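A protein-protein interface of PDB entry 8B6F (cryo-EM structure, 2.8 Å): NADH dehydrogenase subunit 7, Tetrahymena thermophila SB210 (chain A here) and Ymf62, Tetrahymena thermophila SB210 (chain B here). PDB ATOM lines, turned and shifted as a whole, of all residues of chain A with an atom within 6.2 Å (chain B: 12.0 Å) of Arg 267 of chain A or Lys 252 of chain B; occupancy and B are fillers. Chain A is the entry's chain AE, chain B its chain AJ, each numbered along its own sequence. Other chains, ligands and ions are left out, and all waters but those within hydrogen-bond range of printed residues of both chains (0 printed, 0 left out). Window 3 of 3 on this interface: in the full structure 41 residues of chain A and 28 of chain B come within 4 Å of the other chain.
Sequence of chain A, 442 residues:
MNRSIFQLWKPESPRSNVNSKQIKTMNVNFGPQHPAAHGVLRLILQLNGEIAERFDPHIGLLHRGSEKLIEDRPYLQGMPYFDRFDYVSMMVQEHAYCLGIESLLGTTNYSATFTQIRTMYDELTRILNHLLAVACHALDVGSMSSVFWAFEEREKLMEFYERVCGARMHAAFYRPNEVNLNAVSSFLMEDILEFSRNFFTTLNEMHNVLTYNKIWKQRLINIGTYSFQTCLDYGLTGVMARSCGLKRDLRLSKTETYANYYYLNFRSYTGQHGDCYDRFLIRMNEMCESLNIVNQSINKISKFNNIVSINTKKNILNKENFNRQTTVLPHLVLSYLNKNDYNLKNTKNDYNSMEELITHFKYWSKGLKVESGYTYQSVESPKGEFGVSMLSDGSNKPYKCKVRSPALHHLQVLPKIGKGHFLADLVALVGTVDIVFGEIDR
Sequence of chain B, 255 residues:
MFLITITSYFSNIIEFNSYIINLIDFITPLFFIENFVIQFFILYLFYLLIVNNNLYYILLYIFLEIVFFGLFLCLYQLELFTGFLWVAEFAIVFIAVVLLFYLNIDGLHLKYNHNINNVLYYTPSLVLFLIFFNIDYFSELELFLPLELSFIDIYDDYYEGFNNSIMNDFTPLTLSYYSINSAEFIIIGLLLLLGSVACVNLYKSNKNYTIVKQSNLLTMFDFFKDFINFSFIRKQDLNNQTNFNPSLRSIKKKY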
ATOM      1  N   ARG A 251     -28.619  16.477   6.278  1.00  0.00           N
ATOM      2  CA  ARG A 251     -29.626  16.823   7.277  1.00  0.00           C
ATOM      3  C   ARG A 251     -29.163  17.969   8.165  1.00  0.00           C
ATOM      4  O   ARG A 251     -29.984  18.782   8.603  1.00  0.00           O
ATOM      5  CB  ARG A 251     -29.962  15.599   8.129  1.00  0.00           C
ATOM      6  CG  ARG A 251     -30.262  14.352   7.319  1.00  0.00           C
ATOM      7  CD  ARG A 251     -30.814  13.240   8.187  1.00  0.00           C
ATOM      8  NE  ARG A 251     -29.923  12.898   9.289  1.00  0.00           N
ATOM      9  CZ  ARG A 251     -28.917  12.038   9.206  1.00  0.00           C
ATOM     10  NH1 ARG A 251     -28.626  11.419   8.074  1.00  0.00           N
ATOM     11  NH2 ARG A 251     -28.184  11.792  10.287  1.00  0.00           N
ATOM     12  N   LEU A 252     -27.864  18.051   8.440  1.00  0.00           N
ATOM     13  CA  LEU A 252     -27.283  19.086   9.292  1.00  0.00           C
ATOM     14  C   LEU A 252     -26.576  20.157   8.477  1.00  0.00           C
ATOM     15  O   LEU A 252     -25.546  20.692   8.894  1.00  0.00           O
ATOM     16  CB  LEU A 252     -26.326  18.461  10.302  1.00  0.00           C
ATOM     17  CG  LEU A 252     -26.960  17.532  11.336  1.00  0.00           C
ATOM     18  CD1 LEU A 252     -25.900  16.854  12.179  1.00  0.00           C
ATOM     19  CD2 LEU A 252     -27.918  18.312  12.223  1.00  0.00           C
ATOM     20  N   ASN A 265     -30.704  18.145  18.283  1.00  0.00           N
ATOM     21  CA  ASN A 265     -29.311  17.973  18.691  1.00  0.00           C
ATOM     22  C   ASN A 265     -28.979  16.487  18.656  1.00  0.00           C
ATOM     23  O   ASN A 265     -29.076  15.783  19.662  1.00  0.00           O
ATOM     24  CB  ASN A 265     -29.071  18.578  20.069  1.00  0.00           C
ATOM     25  CG  ASN A 265     -29.275  20.077  20.084  1.00  0.00           C
ATOM     26  OD1 ASN A 265     -30.324  20.569  20.496  1.00  0.00           O
ATOM     27  ND2 ASN A 265     -28.272  20.813  19.620  1.00  0.00           N
ATOM     28  N   PHE A 266     -28.583  16.010  17.481  1.00  0.00           N
ATOM     29  CA  PHE A 266     -28.105  14.651  17.293  1.00  0.00           C
ATOM     30  C   PHE A 266     -26.704  14.695  16.699  1.00  0.00           C
ATOM     31  O   PHE A 266     -26.176  15.760  16.368  1.00  0.00           O
ATOM     32  CB  PHE A 266     -29.050  13.841  16.397  1.00  0.00           C
ATOM     33  CG  PHE A 266     -29.181  14.376  15.000  1.00  0.00           C
ATOM     34  CD1 PHE A 266     -30.079  15.389  14.716  1.00  0.00           C
ATOM     35  CD2 PHE A 266     -28.423  13.849  13.968  1.00  0.00           C
ATOM     36  CE1 PHE A 266     -30.209  15.876  13.433  1.00  0.00           C
ATOM     37  CE2 PHE A 266     -28.548  14.332  12.683  1.00  0.00           C
ATOM     38  CZ  PHE A 266     -29.443  15.346  12.413  1.00  0.00           C
ATOM     39  N   ARG A 267     -26.097  13.520  16.571  1.00  0.00           N
ATOM     40  CA  ARG A 267     -24.711  13.397  16.149  1.00  0.00           C
ATOM     41  C   ARG A 267     -24.606  12.505  14.922  1.00  0.00           C
ATOM     42  O   ARG A 267     -25.303  11.492  14.812  1.00  0.00           O
ATOM     43  CB  ARG A 267     -23.850  12.826  17.276  1.00  0.00           C
ATOM     44  CG  ARG A 267     -23.794  13.719  18.501  1.00  0.00           C
ATOM     45  CD  ARG A 267     -23.291  12.972  19.717  1.00  0.00           C
ATOM     46  NE  ARG A 267     -24.190  11.884  20.082  1.00  0.00           N
ATOM     47  CZ  ARG A 267     -24.008  11.078  21.117  1.00  0.00           C
ATOM     48  NH1 ARG A 267     -22.970  11.214  21.924  1.00  0.00           N
ATOM     49  NH2 ARG A 267     -24.891  10.111  21.347  1.00  0.00           N
ATOM     50  N   SER A 268     -23.735  12.898  14.003  1.00  0.00           N
ATOM     51  CA  SER A 268     -23.371  12.098  12.847  1.00  0.00           C
ATOM     52  C   SER A 268     -21.938  11.612  13.012  1.00  0.00           C
ATOM     53  O   SER A 268     -21.094  12.308  13.582  1.00  0.00           O
ATOM     54  CB  SER A 268     -23.516  12.906  11.557  1.00  0.00           C
ATOM     55  OG  SER A 268     -22.998  12.198  10.445  1.00  0.00           O
ATOM     56  N   TYR A 269     -21.669  10.408  12.518  1.00  0.00           N
ATOM     57  CA  TYR A 269     -20.421   9.714  12.793  1.00  0.00           C
ATOM     58  C   TYR A 269     -19.636   9.485  11.510  1.00  0.00           C
ATOM     59  O   TYR A 269     -20.214   9.208  10.455  1.00  0.00           O
ATOM     60  CB  TYR A 269     -20.692   8.384  13.492  1.00  0.00           C
ATOM     61  CG  TYR A 269     -21.554   8.538  14.719  1.00  0.00           C
ATOM     62  CD1 TYR A 269     -22.939   8.525  14.625  1.00  0.00           C
ATOM     63  CD2 TYR A 269     -20.985   8.718  15.972  1.00  0.00           C
ATOM     64  CE1 TYR A 269     -23.732   8.673  15.743  1.00  0.00           C
ATOM     65  CE2 TYR A 269     -21.769   8.867  17.096  1.00  0.00           C
ATOM     66  CZ  TYR A 269     -23.142   8.843  16.975  1.00  0.00           C
ATOM     67  OH  TYR A 269     -23.927   8.991  18.093  1.00  0.00           O
ATOM     68  N   ASN A 285     -23.912   2.771  14.446  1.00  0.00           N
ATOM     69  CA  ASN A 285     -24.069   3.997  15.224  1.00  0.00           C
ATOM     70  C   ASN A 285     -25.235   4.833  14.715  1.00  0.00           C
ATOM     71  O   ASN A 285     -25.965   5.435  15.510  1.00  0.00           O
ATOM     72  CB  ASN A 285     -22.780   4.814  15.195  1.00  0.00           C
ATOM     73  CG  ASN A 285     -21.805   4.392  16.269  1.00  0.00           C
ATOM     74  OD1 ASN A 285     -21.804   3.244  16.706  1.00  0.00           O
ATOM     75  ND2 ASN A 285     -20.976   5.327  16.714  1.00  0.00           N
ATOM     76  N   GLU A 289     -28.397   6.095  16.793  1.00  0.00           N
ATOM     77  CA  GLU A 289     -28.716   7.511  16.915  1.00  0.00           C
ATOM     78  C   GLU A 289     -30.091   7.849  16.360  1.00  0.00           C
ATOM     79  O   GLU A 289     -30.675   8.858  16.765  1.00  0.00           O
ATOM     80  CB  GLU A 289     -27.656   8.352  16.202  1.00  0.00           C
ATOM     81  CG  GLU A 289     -27.721   9.836  16.526  1.00  0.00           C
ATOM     82  CD  GLU A 289     -27.320  10.139  17.955  1.00  0.00           C
ATOM     83  OE1 GLU A 289     -26.918   9.200  18.672  1.00  0.00           O
ATOM     84  OE2 GLU A 289     -27.405  11.315  18.362  1.00  0.00           O
ATOM     85  N   ASN A 292     -32.330   8.132  19.246  1.00  0.00           N
ATOM     86  CA  ASN A 292     -32.283   9.422  19.924  1.00  0.00           C
ATOM     87  C   ASN A 292     -33.057  10.478  19.147  1.00  0.00           C
ATOM     88  O   ASN A 292     -33.776  11.291  19.740  1.00  0.00           O
ATOM     89  CB  ASN A 292     -30.828   9.847  20.120  1.00  0.00           C
ATOM     90  CG  ASN A 292     -30.700  11.158  20.861  1.00  0.00           C
ATOM     91  OD1 ASN A 292     -31.627  11.592  21.540  1.00  0.00           O
ATOM     92  ND2 ASN A 292     -29.543  11.795  20.738  1.00  0.00           N
ATOM     93  N   ILE A 293     -32.926  10.486  17.819  1.00  0.00           N
ATOM     94  CA  ILE A 293     -33.652  11.461  17.009  1.00  0.00           C
ATOM     95  C   ILE A 293     -35.153  11.250  17.146  1.00  0.00           C
ATOM     96  O   ILE A 293     -35.922  12.211  17.272  1.00  0.00           O
ATOM     97  CB  ILE A 293     -33.203  11.383  15.537  1.00  0.00           C
ATOM     98  CG1 ILE A 293     -31.716  11.725  15.420  1.00  0.00           C
ATOM     99  CG2 ILE A 293     -34.024  12.342  14.682  1.00  0.00           C
ATOM    100  CD1 ILE A 293     -31.146  11.536  14.029  1.00  0.00           C
ATOM    101  N   LEU B 248     -15.087   5.386  16.255  1.00  0.00           N
ATOM    102  CA  LEU B 248     -15.659   6.329  15.304  1.00  0.00           C
ATOM    103  C   LEU B 248     -15.479   7.742  15.833  1.00  0.00           C
ATOM    104  O   LEU B 248     -15.296   7.962  17.032  1.00  0.00           O
ATOM    105  CB  LEU B 248     -17.147   6.056  15.044  1.00  0.00           C
ATOM    106  CG  LEU B 248     -17.493   4.830  14.196  1.00  0.00           C
ATOM    107  CD1 LEU B 248     -18.993   4.684  14.091  1.00  0.00           C
ATOM    108  CD2 LEU B 248     -16.879   4.920  12.809  1.00  0.00           C
ATOM    109  N   ARG B 249     -15.534   8.704  14.918  1.00  0.00           N
ATOM    110  CA  ARG B 249     -15.345  10.117  15.236  1.00  0.00           C
ATOM    111  C   ARG B 249     -16.719  10.777  15.309  1.00  0.00           C
ATOM    112  O   ARG B 249     -17.333  11.070  14.280  1.00  0.00           O
ATOM    113  CB  ARG B 249     -14.459  10.779  14.186  1.00  0.00           C
ATOM    114  CG  ARG B 249     -13.951  12.155  14.566  1.00  0.00           C
ATOM    115  CD  ARG B 249     -13.320  12.838  13.362  1.00  0.00           C
ATOM    116  NE  ARG B 249     -12.643  14.081  13.713  1.00  0.00           N
ATOM    117  CZ  ARG B 249     -11.351  14.184  13.995  1.00  0.00           C
ATOM    118  NH1 ARG B 249     -10.554  13.130  13.996  1.00  0.00           N
ATOM    119  NH2 ARG B 249     -10.845  15.380  14.284  1.00  0.00           N
ATOM    120  N   SER B 250     -17.200  11.013  16.526  1.00  0.00           N
ATOM    121  CA  SER B 250     -18.510  11.625  16.707  1.00  0.00           C
ATOM    122  C   SER B 250     -18.456  13.113  16.390  1.00  0.00           C
ATOM    123  O   SER B 250     -17.506  13.809  16.757  1.00  0.00           O
ATOM    124  CB  SER B 250     -19.004  11.420  18.138  1.00  0.00           C
ATOM    125  OG  SER B 250     -19.032  10.047  18.477  1.00  0.00           O
ATOM    126  N   ILE B 251     -19.493  13.603  15.717  1.00  0.00           N
ATOM    127  CA  ILE B 251     -19.596  15.002  15.322  1.00  0.00           C
ATOM    128  C   ILE B 251     -20.905  15.555  15.866  1.00  0.00           C
ATOM    129  O   ILE B 251     -21.961  14.934  15.702  1.00  0.00           O
ATOM    130  CB  ILE B 251     -19.529  15.172  13.794  1.00  0.00           C
ATOM    131  CG1 ILE B 251     -18.363  14.371  13.205  1.00  0.00           C
ATOM    132  CG2 ILE B 251     -19.401  16.643  13.434  1.00  0.00           C
ATOM    133  CD1 ILE B 251     -16.991  14.826  13.663  1.00  0.00           C
ATOM    134  N   LYS B 252     -20.834  16.714  16.514  1.00  0.00           N
ATOM    135  CA  LYS B 252     -22.003  17.412  17.025  1.00  0.00           C
ATOM    136  C   LYS B 252     -21.912  18.881  16.640  1.00  0.00           C
ATOM    137  O   LYS B 252     -20.893  19.353  16.128  1.00  0.00           O
ATOM    138  CB  LYS B 252     -22.126  17.266  18.548  1.00  0.00           C
ATOM    139  CG  LYS B 252     -20.903  17.736  19.320  1.00  0.00           C
ATOM    140  CD  LYS B 252     -21.173  17.793  20.819  1.00  0.00           C
ATOM    141  CE  LYS B 252     -21.537  16.430  21.381  1.00  0.00           C
ATOM    142  NZ  LYS B 252     -21.691  16.472  22.861  1.00  0.00           N
ATOM    143  N   LYS B 253     -22.995  19.611  16.889  1.00  0.00           N
ATOM    144  CA  LYS B 253     -23.023  21.031  16.581  1.00  0.00           C
ATOM    145  C   LYS B 253     -22.086  21.804  17.506  1.00  0.00           C
ATOM    146  O   LYS B 253     -21.752  21.365  18.611  1.00  0.00           O
ATOM    147  CB  LYS B 253     -24.444  21.579  16.706  1.00  0.00           C
ATOM    148  CG  LYS B 253     -25.406  21.025  15.673  1.00  0.00           C
ATOM    149  CD  LYS B 253     -26.781  21.654  15.811  1.00  0.00           C
ATOM    150  CE  LYS B 253     -27.702  21.222  14.685  1.00  0.00           C
ATOM    151  NZ  LYS B 253     -27.194  21.654  13.353  1.00  0.00           N
ATOM    152  N   LYS B 254     -21.663  22.974  17.037  1.00  0.00           N
ATOM    153  CA  LYS B 254     -20.768  23.813  17.820  1.00  0.00           C
ATOM    154  C   LYS B 254     -21.444  24.254  19.111  1.00  0.00           C
ATOM    155  O   LYS B 254     -22.653  24.493  19.149  1.00  0.00           O
ATOM    156  CB  LYS B 254     -20.348  25.039  17.009  1.00  0.00           C
ATOM    157  CG  LYS B 254     -19.617  24.718  15.718  1.00  0.00           C
ATOM    158  CD  LYS B 254     -19.383  25.976  14.896  1.00  0.00           C
ATOM    159  CE  LYS B 254     -18.669  25.660  13.594  1.00  0.00           C
ATOM    160  NZ  LYS B 254     -18.430  26.882  12.778  1.00  0.00           N
ATOM    161  N   TYR B 255     -20.654  24.359  20.174  1.00  0.00           N
ATOM    162  CA  TYR B 255     -21.154  24.829  21.460  1.00  0.00           C
ATOM    163  C   TYR B 255     -20.233  25.903  22.029  1.00  0.00           C
ATOM    164  O   TYR B 255     -19.080  26.032  21.618  1.00  0.00           O
ATOM    165  CB  TYR B 255     -21.287  23.666  22.445  1.00  0.00           C
ATOM    166  CG  TYR B 255     -19.996  22.922  22.691  1.00  0.00           C
ATOM    167  CD1 TYR B 255     -19.119  23.323  23.691  1.00  0.00           C
ATOM    168  CD2 TYR B 255     -19.656  21.817  21.924  1.00  0.00           C
ATOM    169  CE1 TYR B 255     -17.938  22.643  23.919  1.00  0.00           C
ATOM    170  CE2 TYR B 255     -18.477  21.131  22.143  1.00  0.00           C
ATOM    171  CZ  TYR B 255     -17.622  21.548  23.142  1.00  0.00           C
ATOM    172  OH  TYR B 255     -16.447  20.869  23.364  1.00  0.00           O
ATOM    173  OXT TYR B 255     -20.618  26.673  22.908  1.00  0.00           O
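The backbone NH of Ile 251 of chain B is in hydrogen-bond range of the backbone carbonyl oxygen of Ser 268 of chain A, 3.0 Å away.
The guanidinium group (NH2) of Arg 267 of chain A is in salt-bridge range of the side-chain carboxylate (OE1) of Glu 289 of chain A, 3.5 Å away. OE1 of Glu 289 of chain A lies within hydrogen-bond range of OH of Tyr 269 of chain A, at 3.1 Å.
Among the printed residues, merely in contact across the chains: Arg 267 of chain A with Ile 251 of chain B, Tyr 269 of chain A with Ser 250 of chain B, Asn 285 of chain A with Leu 248 of chain B, Leu 252 of chain A with Lys 253 of chain B, Tyr 269 of chain A with Arg 249 of chain B, Arg 267 of chain A with Lys 252 of chain B and Ser 268 of chain A with Ser 250 of chain B.
Arg 267 of chain A touches just these residues of chain B: Ile 251 and Lys 252. Lys 252 of chain B touches one residue of chain A. Of the printed residues of chain B, Ser 268 of chain A touches Ser 250 and Ile 251. Tyr 269 of chain A touches two residues of chain B. No residue of chain B comes within 4 Å of Glu 289 of chain A. Of the printed residues of chain A, Leu 248 of chain B touches Asn 285. Printed residues of chain A within 4 Å of Arg 249 of chain B: Tyr 269 (3.7 Å). Asn 265 of chain A touches none of the printed residues of chain B. Lys 254 of chain B touches none of the printed residues of chain A. The nearest residue of chain A that does not touch Lys 252 of chain B is Phe 266 of chain A (4.5 Å).
Hydrophobic or aromatic side chains of chain B that line the printed part of chain A: Leu 248 and Ile 251. Of the 11 printed residues of chain A, 5 touch a printed residue of chain B. Among the printed residues, no Asp or Glu carboxylate lies within 4 Å of a Lys or Arg side-chain nitrogen of the other chain.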
